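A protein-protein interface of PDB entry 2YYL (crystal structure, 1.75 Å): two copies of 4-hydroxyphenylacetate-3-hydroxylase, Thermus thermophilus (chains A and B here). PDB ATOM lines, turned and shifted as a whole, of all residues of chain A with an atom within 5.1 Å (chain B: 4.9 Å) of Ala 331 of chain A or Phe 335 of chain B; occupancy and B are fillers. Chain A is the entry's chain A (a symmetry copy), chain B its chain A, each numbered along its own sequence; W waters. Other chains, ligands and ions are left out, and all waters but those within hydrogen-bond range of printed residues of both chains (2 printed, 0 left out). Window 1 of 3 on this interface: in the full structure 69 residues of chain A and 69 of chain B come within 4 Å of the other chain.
OE2 of Glu 330 of chain A is in salt-bridge range of NH1 of Arg 333 of chain A, at 2.9 Å.
Among the printed residues, pairs that only touch across the chains: Glu 330 of chain A with Ala 357 of chain B (3.5 Å), Phe 335 of chain A with Ala 331 of chain B (3.5 Å), Ala 331 of chain A with Phe 335 of chain B (3.5 Å), Ala 334 of chain A with Ala 334 of chain B (3.5 Å), Ala 334 of chain A with Phe 335 of chain B (3.7 Å), Phe 335 of chain A with Ala 334 of chain B (3.7 Å), Ala 334 of chain A with Arg 338 of chain B (3.7 Å), Glu 330 of chain A with Phe 335 of chain B (3.7 Å), Arg 333 of chain A with Arg 338 of chain B (3.8 Å), Val 327 of chain A with Leu 364 of chain B (3.8 Å) and Val 327 of chain A with Gly 360 of chain B (3.8 Å).
Ala 331 of chain A touches one residue of chain B. Of the printed residues of chain B, Arg 333 of chain A touches Arg 338. Of the printed residues of chain B, Phe 335 of chain A touches Ala 331 and Ala 334. Of chain A, only Glu 330, Ala 331 and Ala 334 come within 4 Å of Phe 335 of chain B. Of the printed residues of chain A, Ala 357 of chain B touches Glu 330. Printed residues of chain A within 4 Å of Gly 360 of chain B: Val 327. Printed residues of chain A within 4 Å of Leu 364 of chain B: Val 327 (3.8 Å).
Of the 14 printed residues of chain B, 7 touch a printed residue of chain A. Hydrophobic or aromatic side chains of chain B within 4 Å of the printed part of chain A: Ala 331, Ala 334, Phe 335 and Leu 364. Of the 12 printed residues of chain A, 6 touch a printed residue of chain B. Hydrophobic or aromatic side chains of chain A that line the printed part of chain B: Val 327, Ala 331, Ala 334 and Phe 335. Among the printed residues, no Asp or Glu carboxylate lies within 4 Å of a Lys or Arg side-chain nitrogen of the other chain.
Ala 331 of chain A touches Phe 335 of chain B, and with the chains exchanged Phe 335 of chain A touches Ala 331 of chain B. Ala 334 of chain B touches its own counterpart, Ala 334 of chain A. Ala 334 of chain A touches Phe 335 of chain B, and with the chains exchanged Phe 335 of chain A touches Ala 334 of chain B. Of the 11 pairs that touch across the chains among the printed residues, 5 have their exchanged pair printed and touching as well.
Water W2 lies within hydrogen-bond range of OE1 of Glu 330 of chain A (2.7 Å) and NE of Arg 338 of chain B (2.8 Å). Water W1 bridges the side-chain carboxylate (OE1) of Glu 330 of chain A (2.7 Å) and the guanidinium group (NE) of Arg 338 of chain B (3.4 Å).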
ATOM      1  N   ILE A 326      10.001   7.180  20.156  1.00  0.00           N
ATOM      2  CA  ILE A 326       8.924   6.200  20.258  1.00  0.00           C
ATOM      3  C   ILE A 326       8.443   5.796  18.864  1.00  0.00           C
ATOM      4  O   ILE A 326       8.186   4.620  18.600  1.00  0.00           O
ATOM      5  CB  ILE A 326       7.739   6.765  21.078  1.00  0.00           C
ATOM      6  CG1 ILE A 326       8.142   6.854  22.554  1.00  0.00           C
ATOM      7  CG2 ILE A 326       6.503   5.876  20.909  1.00  0.00           C
ATOM      8  CD1 ILE A 326       7.183   7.659  23.419  1.00  0.00           C
ATOM      9  N   VAL A 327       8.324   6.776  17.975  1.00  0.00           N
ATOM     10  CA  VAL A 327       7.891   6.502  16.610  1.00  0.00           C
ATOM     11  C   VAL A 327       8.897   5.569  15.936  1.00  0.00           C
ATOM     12  O   VAL A 327       8.517   4.592  15.285  1.00  0.00           O
ATOM     13  CB  VAL A 327       7.771   7.815  15.792  1.00  0.00           C
ATOM     14  CG1 VAL A 327       7.586   7.512  14.303  1.00  0.00           C
ATOM     15  CG2 VAL A 327       6.600   8.635  16.316  1.00  0.00           C
ATOM     16  N   TYR A 328      10.183   5.856  16.099  1.00  0.00           N
ATOM     17  CA  TYR A 328      11.204   5.014  15.482  1.00  0.00           C
ATOM     18  C   TYR A 328      11.195   3.619  16.087  1.00  0.00           C
ATOM     19  O   TYR A 328      11.385   2.631  15.378  1.00  0.00           O
ATOM     20  CB  TYR A 328      12.590   5.650  15.625  1.00  0.00           C
ATOM     21  CG  TYR A 328      12.672   7.042  15.027  1.00  0.00           C
ATOM     22  CD1 TYR A 328      11.837   7.419  13.976  1.00  0.00           C
ATOM     23  CD2 TYR A 328      13.597   7.973  15.500  1.00  0.00           C
ATOM     24  CE1 TYR A 328      11.918   8.692  13.410  1.00  0.00           C
ATOM     25  CE2 TYR A 328      13.688   9.249  14.941  1.00  0.00           C
ATOM     26  CZ  TYR A 328      12.845   9.598  13.898  1.00  0.00           C
ATOM     27  OH  TYR A 328      12.931  10.857  13.346  1.00  0.00           O
ATOM     28  N   LEU A 329      10.975   3.539  17.397  1.00  0.00           N
ATOM     29  CA  LEU A 329      10.914   2.242  18.067  1.00  0.00           C
ATOM     30  C   LEU A 329       9.782   1.420  17.454  1.00  0.00           C
ATOM     31  O   LEU A 329       9.959   0.245  17.120  1.00  0.00           O
ATOM     32  CB  LEU A 329      10.646   2.422  19.564  1.00  0.00           C
ATOM     33  CG  LEU A 329      10.308   1.135  20.328  1.00  0.00           C
ATOM     34  CD1 LEU A 329      11.448   0.124  20.159  1.00  0.00           C
ATOM     35  CD2 LEU A 329      10.086   1.450  21.800  1.00  0.00           C
ATOM     36  N   GLU A 330       8.610   2.031  17.315  1.00  0.00           N
ATOM     37  CA  GLU A 330       7.473   1.327  16.737  1.00  0.00           C
ATOM     38  C   GLU A 330       7.734   0.929  15.282  1.00  0.00           C
ATOM     39  O   GLU A 330       7.297  -0.130  14.834  1.00  0.00           O
ATOM     40  CB  GLU A 330       6.205   2.182  16.849  1.00  0.00           C
ATOM     41  CG  GLU A 330       5.694   2.333  18.282  1.00  0.00           C
ATOM     42  CD  GLU A 330       5.220   1.012  18.882  1.00  0.00           C
ATOM     43  OE1 GLU A 330       4.717   0.161  18.125  1.00  0.00           O
ATOM     44  OE2 GLU A 330       5.328   0.828  20.112  1.00  0.00           O
ATOM     45  N   ALA A 331       8.451   1.768  14.542  1.00  0.00           N
ATOM     46  CA  ALA A 331       8.758   1.444  13.154  1.00  0.00           C
ATOM     47  C   ALA A 331       9.582   0.155  13.100  1.00  0.00           C
ATOM     48  O   ALA A 331       9.314  -0.731  12.288  1.00  0.00           O
ATOM     49  CB  ALA A 331       9.531   2.588  12.499  1.00  0.00           C
ATOM     50  N   MET A 332      10.577   0.043  13.973  1.00  0.00           N
ATOM     51  CA  MET A 332      11.421  -1.148  13.978  1.00  0.00           C
ATOM     52  C   MET A 332      10.632  -2.377  14.425  1.00  0.00           C
ATOM     53  O   MET A 332      10.823  -3.470  13.888  1.00  0.00           O
ATOM     54  CB  MET A 332      12.646  -0.927  14.870  1.00  0.00           C
ATOM     55  CG  MET A 332      13.556   0.200  14.381  1.00  0.00           C
ATOM     56  SD  MET A 332      14.040   0.022  12.634  1.00  0.00           S
ATOM     57  CE  MET A 332      15.329  -1.161  12.777  1.00  0.00           C
ATOM     58  N   ARG A 333       9.742  -2.202  15.401  1.00  0.00           N
ATOM     59  CA  ARG A 333       8.916  -3.313  15.861  1.00  0.00           C
ATOM     60  C   ARG A 333       8.024  -3.781  14.719  1.00  0.00           C
ATOM     61  O   ARG A 333       7.789  -4.980  14.553  1.00  0.00           O
ATOM     62  CB  ARG A 333       8.038  -2.883  17.033  1.00  0.00           C
ATOM     63  CG  ARG A 333       8.756  -2.860  18.364  1.00  0.00           C
ATOM     64  CD  ARG A 333       7.854  -2.307  19.454  1.00  0.00           C
ATOM     65  NE  ARG A 333       8.504  -2.375  20.759  1.00  0.00           N
ATOM     66  CZ  ARG A 333       8.116  -1.681  21.821  1.00  0.00           C
ATOM     67  NH1 ARG A 333       7.077  -0.861  21.739  1.00  0.00           N
ATOM     68  NH2 ARG A 333       8.779  -1.800  22.964  1.00  0.00           N
ATOM     69  N   ALA A 334       7.528  -2.829  13.936  1.00  0.00           N
ATOM     70  CA  ALA A 334       6.653  -3.156  12.814  1.00  0.00           C
ATOM     71  C   ALA A 334       7.397  -3.960  11.751  1.00  0.00           C
ATOM     72  O   ALA A 334       6.877  -4.958  11.256  1.00  0.00           O
ATOM     73  CB  ALA A 334       6.067  -1.877  12.211  1.00  0.00           C
ATOM     74  N   PHE A 335       8.610  -3.530  11.404  1.00  0.00           N
ATOM     75  CA  PHE A 335       9.405  -4.246  10.406  1.00  0.00           C
ATOM     76  C   PHE A 335       9.646  -5.679  10.878  1.00  0.00           C
ATOM     77  O   PHE A 335       9.551  -6.629  10.105  1.00  0.00           O
ATOM     78  CB  PHE A 335      10.763  -3.563  10.203  1.00  0.00           C
ATOM     79  CG  PHE A 335      10.723  -2.367   9.290  1.00  0.00           C
ATOM     80  CD1 PHE A 335      10.137  -2.457   8.032  1.00  0.00           C
ATOM     81  CD2 PHE A 335      11.335  -1.171   9.664  1.00  0.00           C
ATOM     82  CE1 PHE A 335      10.168  -1.375   7.148  1.00  0.00           C
ATOM     83  CE2 PHE A 335      11.371  -0.083   8.789  1.00  0.00           C
ATOM     84  CZ  PHE A 335      10.786  -0.188   7.530  1.00  0.00           C
ATOM     85  N   LEU A 364      16.583   1.870   6.739  1.00  0.00           N
ATOM     86  CA  LEU A 364      16.005   3.010   7.423  1.00  0.00           C
ATOM     87  C   LEU A 364      16.747   3.309   8.725  1.00  0.00           C
ATOM     88  O   LEU A 364      17.052   4.464   9.016  1.00  0.00           O
ATOM     89  CB  LEU A 364      14.518   2.779   7.730  1.00  0.00           C
ATOM     90  CG  LEU A 364      13.826   3.983   8.386  1.00  0.00           C
ATOM     91  CD1 LEU A 364      13.853   5.180   7.428  1.00  0.00           C
ATOM     92  CD2 LEU A 364      12.390   3.625   8.744  1.00  0.00           C
ATOM     93  N   LEU A 368      17.898   6.704  10.950  1.00  0.00           N
ATOM     94  CA  LEU A 368      17.261   7.038  12.223  1.00  0.00           C
ATOM     95  C   LEU A 368      18.237   7.143  13.393  1.00  0.00           C
ATOM     96  O   LEU A 368      18.091   8.020  14.248  1.00  0.00           O
ATOM     97  CB  LEU A 368      16.198   5.995  12.584  1.00  0.00           C
ATOM     98  CG  LEU A 368      15.105   5.691  11.558  1.00  0.00           C
ATOM     99  CD1 LEU A 368      14.142   4.667  12.144  1.00  0.00           C
ATOM    100  CD2 LEU A 368      14.363   6.971  11.195  1.00  0.00           C
ATOM    101  N   VAL B 289      -3.600   4.105   7.403  1.00  0.00           N
ATOM    102  CA  VAL B 289      -2.364   3.423   7.031  1.00  0.00           C
ATOM    103  C   VAL B 289      -2.523   2.690   5.694  1.00  0.00           C
ATOM    104  O   VAL B 289      -1.599   2.664   4.885  1.00  0.00           O
ATOM    105  CB  VAL B 289      -1.878   2.458   8.150  1.00  0.00           C
ATOM    106  CG1 VAL B 289      -2.777   1.244   8.242  1.00  0.00           C
ATOM    107  CG2 VAL B 289      -0.430   2.046   7.885  1.00  0.00           C
ATOM    108  N   ALA B 331       7.864   0.619   5.185  1.00  0.00           N
ATOM    109  CA  ALA B 331       7.611   1.040   6.558  1.00  0.00           C
ATOM    110  C   ALA B 331       6.101   1.092   6.808  1.00  0.00           C
ATOM    111  O   ALA B 331       5.615   0.617   7.834  1.00  0.00           O
ATOM    112  CB  ALA B 331       8.232   2.412   6.817  1.00  0.00           C
ATOM    113  N   MET B 332       5.357   1.657   5.863  1.00  0.00           N
ATOM    114  CA  MET B 332       3.911   1.760   6.029  1.00  0.00           C
ATOM    115  C   MET B 332       3.254   0.382   5.994  1.00  0.00           C
ATOM    116  O   MET B 332       2.313   0.119   6.744  1.00  0.00           O
ATOM    117  CB  MET B 332       3.318   2.680   4.957  1.00  0.00           C
ATOM    118  CG  MET B 332       3.829   4.118   5.042  1.00  0.00           C
ATOM    119  SD  MET B 332       3.649   4.845   6.702  1.00  0.00           S
ATOM    120  CE  MET B 332       1.951   5.290   6.676  1.00  0.00           C
ATOM    121  N   ARG B 333       3.751  -0.502   5.129  1.00  0.00           N
ATOM    122  CA  ARG B 333       3.212  -1.855   5.058  1.00  0.00           C
ATOM    123  C   ARG B 333       3.453  -2.562   6.384  1.00  0.00           C
ATOM    124  O   ARG B 333       2.604  -3.320   6.859  1.00  0.00           O
ATOM    125  CB  ARG B 333       3.889  -2.648   3.942  1.00  0.00           C
ATOM    126  CG  ARG B 333       3.347  -2.354   2.562  1.00  0.00           C
ATOM    127  CD  ARG B 333       4.150  -3.085   1.499  1.00  0.00           C
ATOM    128  NE  ARG B 333       3.572  -2.887   0.175  1.00  0.00           N
ATOM    129  CZ  ARG B 333       4.219  -3.113  -0.962  1.00  0.00           C
ATOM    130  NH1 ARG B 333       5.473  -3.547  -0.941  1.00  0.00           N
ATOM    131  NH2 ARG B 333       3.613  -2.892  -2.120  1.00  0.00           N
ATOM    132  N   ALA B 334       4.616  -2.312   6.978  1.00  0.00           N
ATOM    133  CA  ALA B 334       4.962  -2.938   8.250  1.00  0.00           C
ATOM    134  C   ALA B 334       4.032  -2.471   9.366  1.00  0.00           C
ATOM    135  O   ALA B 334       3.546  -3.287  10.147  1.00  0.00           O
ATOM    136  CB  ALA B 334       6.421  -2.641   8.605  1.00  0.00           C
ATOM    137  N   PHE B 335       3.782  -1.164   9.440  1.00  0.00           N
ATOM    138  CA  PHE B 335       2.888  -0.625  10.465  1.00  0.00           C
ATOM    139  C   PHE B 335       1.504  -1.255  10.319  1.00  0.00           C
ATOM    140  O   PHE B 335       0.865  -1.628  11.300  1.00  0.00           O
ATOM    141  CB  PHE B 335       2.751   0.895  10.321  1.00  0.00           C
ATOM    142  CG  PHE B 335       3.888   1.678  10.922  1.00  0.00           C
ATOM    143  CD1 PHE B 335       4.293   1.444  12.232  1.00  0.00           C
ATOM    144  CD2 PHE B 335       4.503   2.699  10.199  1.00  0.00           C
ATOM    145  CE1 PHE B 335       5.293   2.221  12.822  1.00  0.00           C
ATOM    146  CE2 PHE B 335       5.504   3.482  10.779  1.00  0.00           C
ATOM    147  CZ  PHE B 335       5.897   3.241  12.093  1.00  0.00           C
ATOM    148  N   TRP B 336       1.053  -1.358   9.077  1.00  0.00           N
ATOM    149  CA  TRP B 336      -0.253  -1.935   8.760  1.00  0.00           C
ATOM    150  C   TRP B 336      -0.313  -3.386   9.245  1.00  0.00           C
ATOM    151  O   TRP B 336      -1.249  -3.783   9.944  1.00  0.00           O
ATOM    152  CB  TRP B 336      -0.457  -1.848   7.244  1.00  0.00           C
ATOM    153  CG  TRP B 336      -1.779  -2.297   6.703  1.00  0.00           C
ATOM    154  CD1 TRP B 336      -2.821  -2.861   7.387  1.00  0.00           C
ATOM    155  CD2 TRP B 336      -2.173  -2.260   5.328  1.00  0.00           C
ATOM    156  NE1 TRP B 336      -3.840  -3.182   6.514  1.00  0.00           N
ATOM    157  CE2 TRP B 336      -3.465  -2.824   5.246  1.00  0.00           C
ATOM    158  CE3 TRP B 336      -1.552  -1.807   4.154  1.00  0.00           C
ATOM    159  CZ2 TRP B 336      -4.151  -2.946   4.029  1.00  0.00           C
ATOM    160  CZ3 TRP B 336      -2.234  -1.928   2.945  1.00  0.00           C
ATOM    161  CH2 TRP B 336      -3.521  -2.495   2.894  1.00  0.00           C
ATOM    162  N   THR B 337       0.692  -4.178   8.890  1.00  0.00           N
ATOM    163  CA  THR B 337       0.717  -5.574   9.312  1.00  0.00           C
ATOM    164  C   THR B 337       0.715  -5.706  10.833  1.00  0.00           C
ATOM    165  O   THR B 337      -0.081  -6.453  11.390  1.00  0.00           O
ATOM    166  CB  THR B 337       1.950  -6.308   8.737  1.00  0.00           C
ATOM    167  OG1 THR B 337       1.812  -6.411   7.316  1.00  0.00           O
ATOM    168  CG2 THR B 337       2.074  -7.707   9.331  1.00  0.00           C
ATOM    169  N   ARG B 338       1.587  -4.969  11.516  1.00  0.00           N
ATOM    170  CA  ARG B 338       1.634  -5.084  12.970  1.00  0.00           C
ATOM    171  C   ARG B 338       0.356  -4.578  13.635  1.00  0.00           C
ATOM    172  O   ARG B 338      -0.054  -5.101  14.669  1.00  0.00           O
ATOM    173  CB  ARG B 338       2.847  -4.340  13.539  1.00  0.00           C
ATOM    174  CG  ARG B 338       3.023  -4.535  15.042  1.00  0.00           C
ATOM    175  CD  ARG B 338       4.306  -3.886  15.560  1.00  0.00           C
ATOM    176  NE  ARG B 338       4.319  -3.845  17.023  1.00  0.00           N
ATOM    177  CZ  ARG B 338       4.721  -4.839  17.806  1.00  0.00           C
ATOM    178  NH1 ARG B 338       5.161  -5.977  17.278  1.00  0.00           N
ATOM    179  NH2 ARG B 338       4.666  -4.699  19.125  1.00  0.00           N
ATOM    180  N   ALA B 339      -0.272  -3.567  13.044  1.00  0.00           N
ATOM    181  CA  ALA B 339      -1.500  -3.022  13.612  1.00  0.00           C
ATOM    182  C   ALA B 339      -2.569  -4.111  13.673  1.00  0.00           C
ATOM    183  O   ALA B 339      -3.322  -4.202  14.643  1.00  0.00           O
ATOM    184  CB  ALA B 339      -1.996  -1.844  12.771  1.00  0.00           C
ATOM    185  N   ALA B 357       1.490   0.680  16.799  1.00  0.00           N
ATOM    186  CA  ALA B 357       1.818   0.664  15.380  1.00  0.00           C
ATOM    187  C   ALA B 357       1.137   1.791  14.614  1.00  0.00           C
ATOM    188  O   ALA B 357       1.745   2.412  13.737  1.00  0.00           O
ATOM    189  CB  ALA B 357       1.431  -0.684  14.773  1.00  0.00           C
ATOM    190  N   GLY B 360       2.575   5.112  15.352  1.00  0.00           N
ATOM    191  CA  GLY B 360       3.842   5.223  14.653  1.00  0.00           C
ATOM    192  C   GLY B 360       3.588   5.647  13.215  1.00  0.00           C
ATOM    193  O   GLY B 360       4.227   6.567  12.702  1.00  0.00           O
ATOM    194  N   ALA B 361       2.637   4.983  12.565  1.00  0.00           N
ATOM    195  CA  ALA B 361       2.318   5.283  11.172  1.00  0.00           C
ATOM    196  C   ALA B 361       1.789   6.695  10.933  1.00  0.00           C
ATOM    197  O   ALA B 361       2.230   7.376  10.003  1.00  0.00           O
ATOM    198  CB  ALA B 361       1.306   4.258  10.638  1.00  0.00           C
ATOM    199  N   LEU B 364       4.589   9.283  11.606  1.00  0.00           N
ATOM    200  CA  LEU B 364       5.760   9.212  10.754  1.00  0.00           C
ATOM    201  C   LEU B 364       5.438   9.672   9.332  1.00  0.00           C
ATOM    202  O   LEU B 364       6.196  10.436   8.739  1.00  0.00           O
ATOM    203  CB  LEU B 364       6.329   7.786  10.708  1.00  0.00           C
ATOM    204  CG  LEU B 364       7.617   7.659   9.883  1.00  0.00           C
ATOM    205  CD1 LEU B 364       8.724   8.508  10.518  1.00  0.00           C
ATOM    206  CD2 LEU B 364       8.046   6.200   9.811  1.00  0.00           C
HETATM  207  O   HOH W   1       4.719  -0.766  15.539  1.00  0.00           O
HETATM  208  O   HOH W   2       3.298  -2.047  18.897  1.00  0.00           O
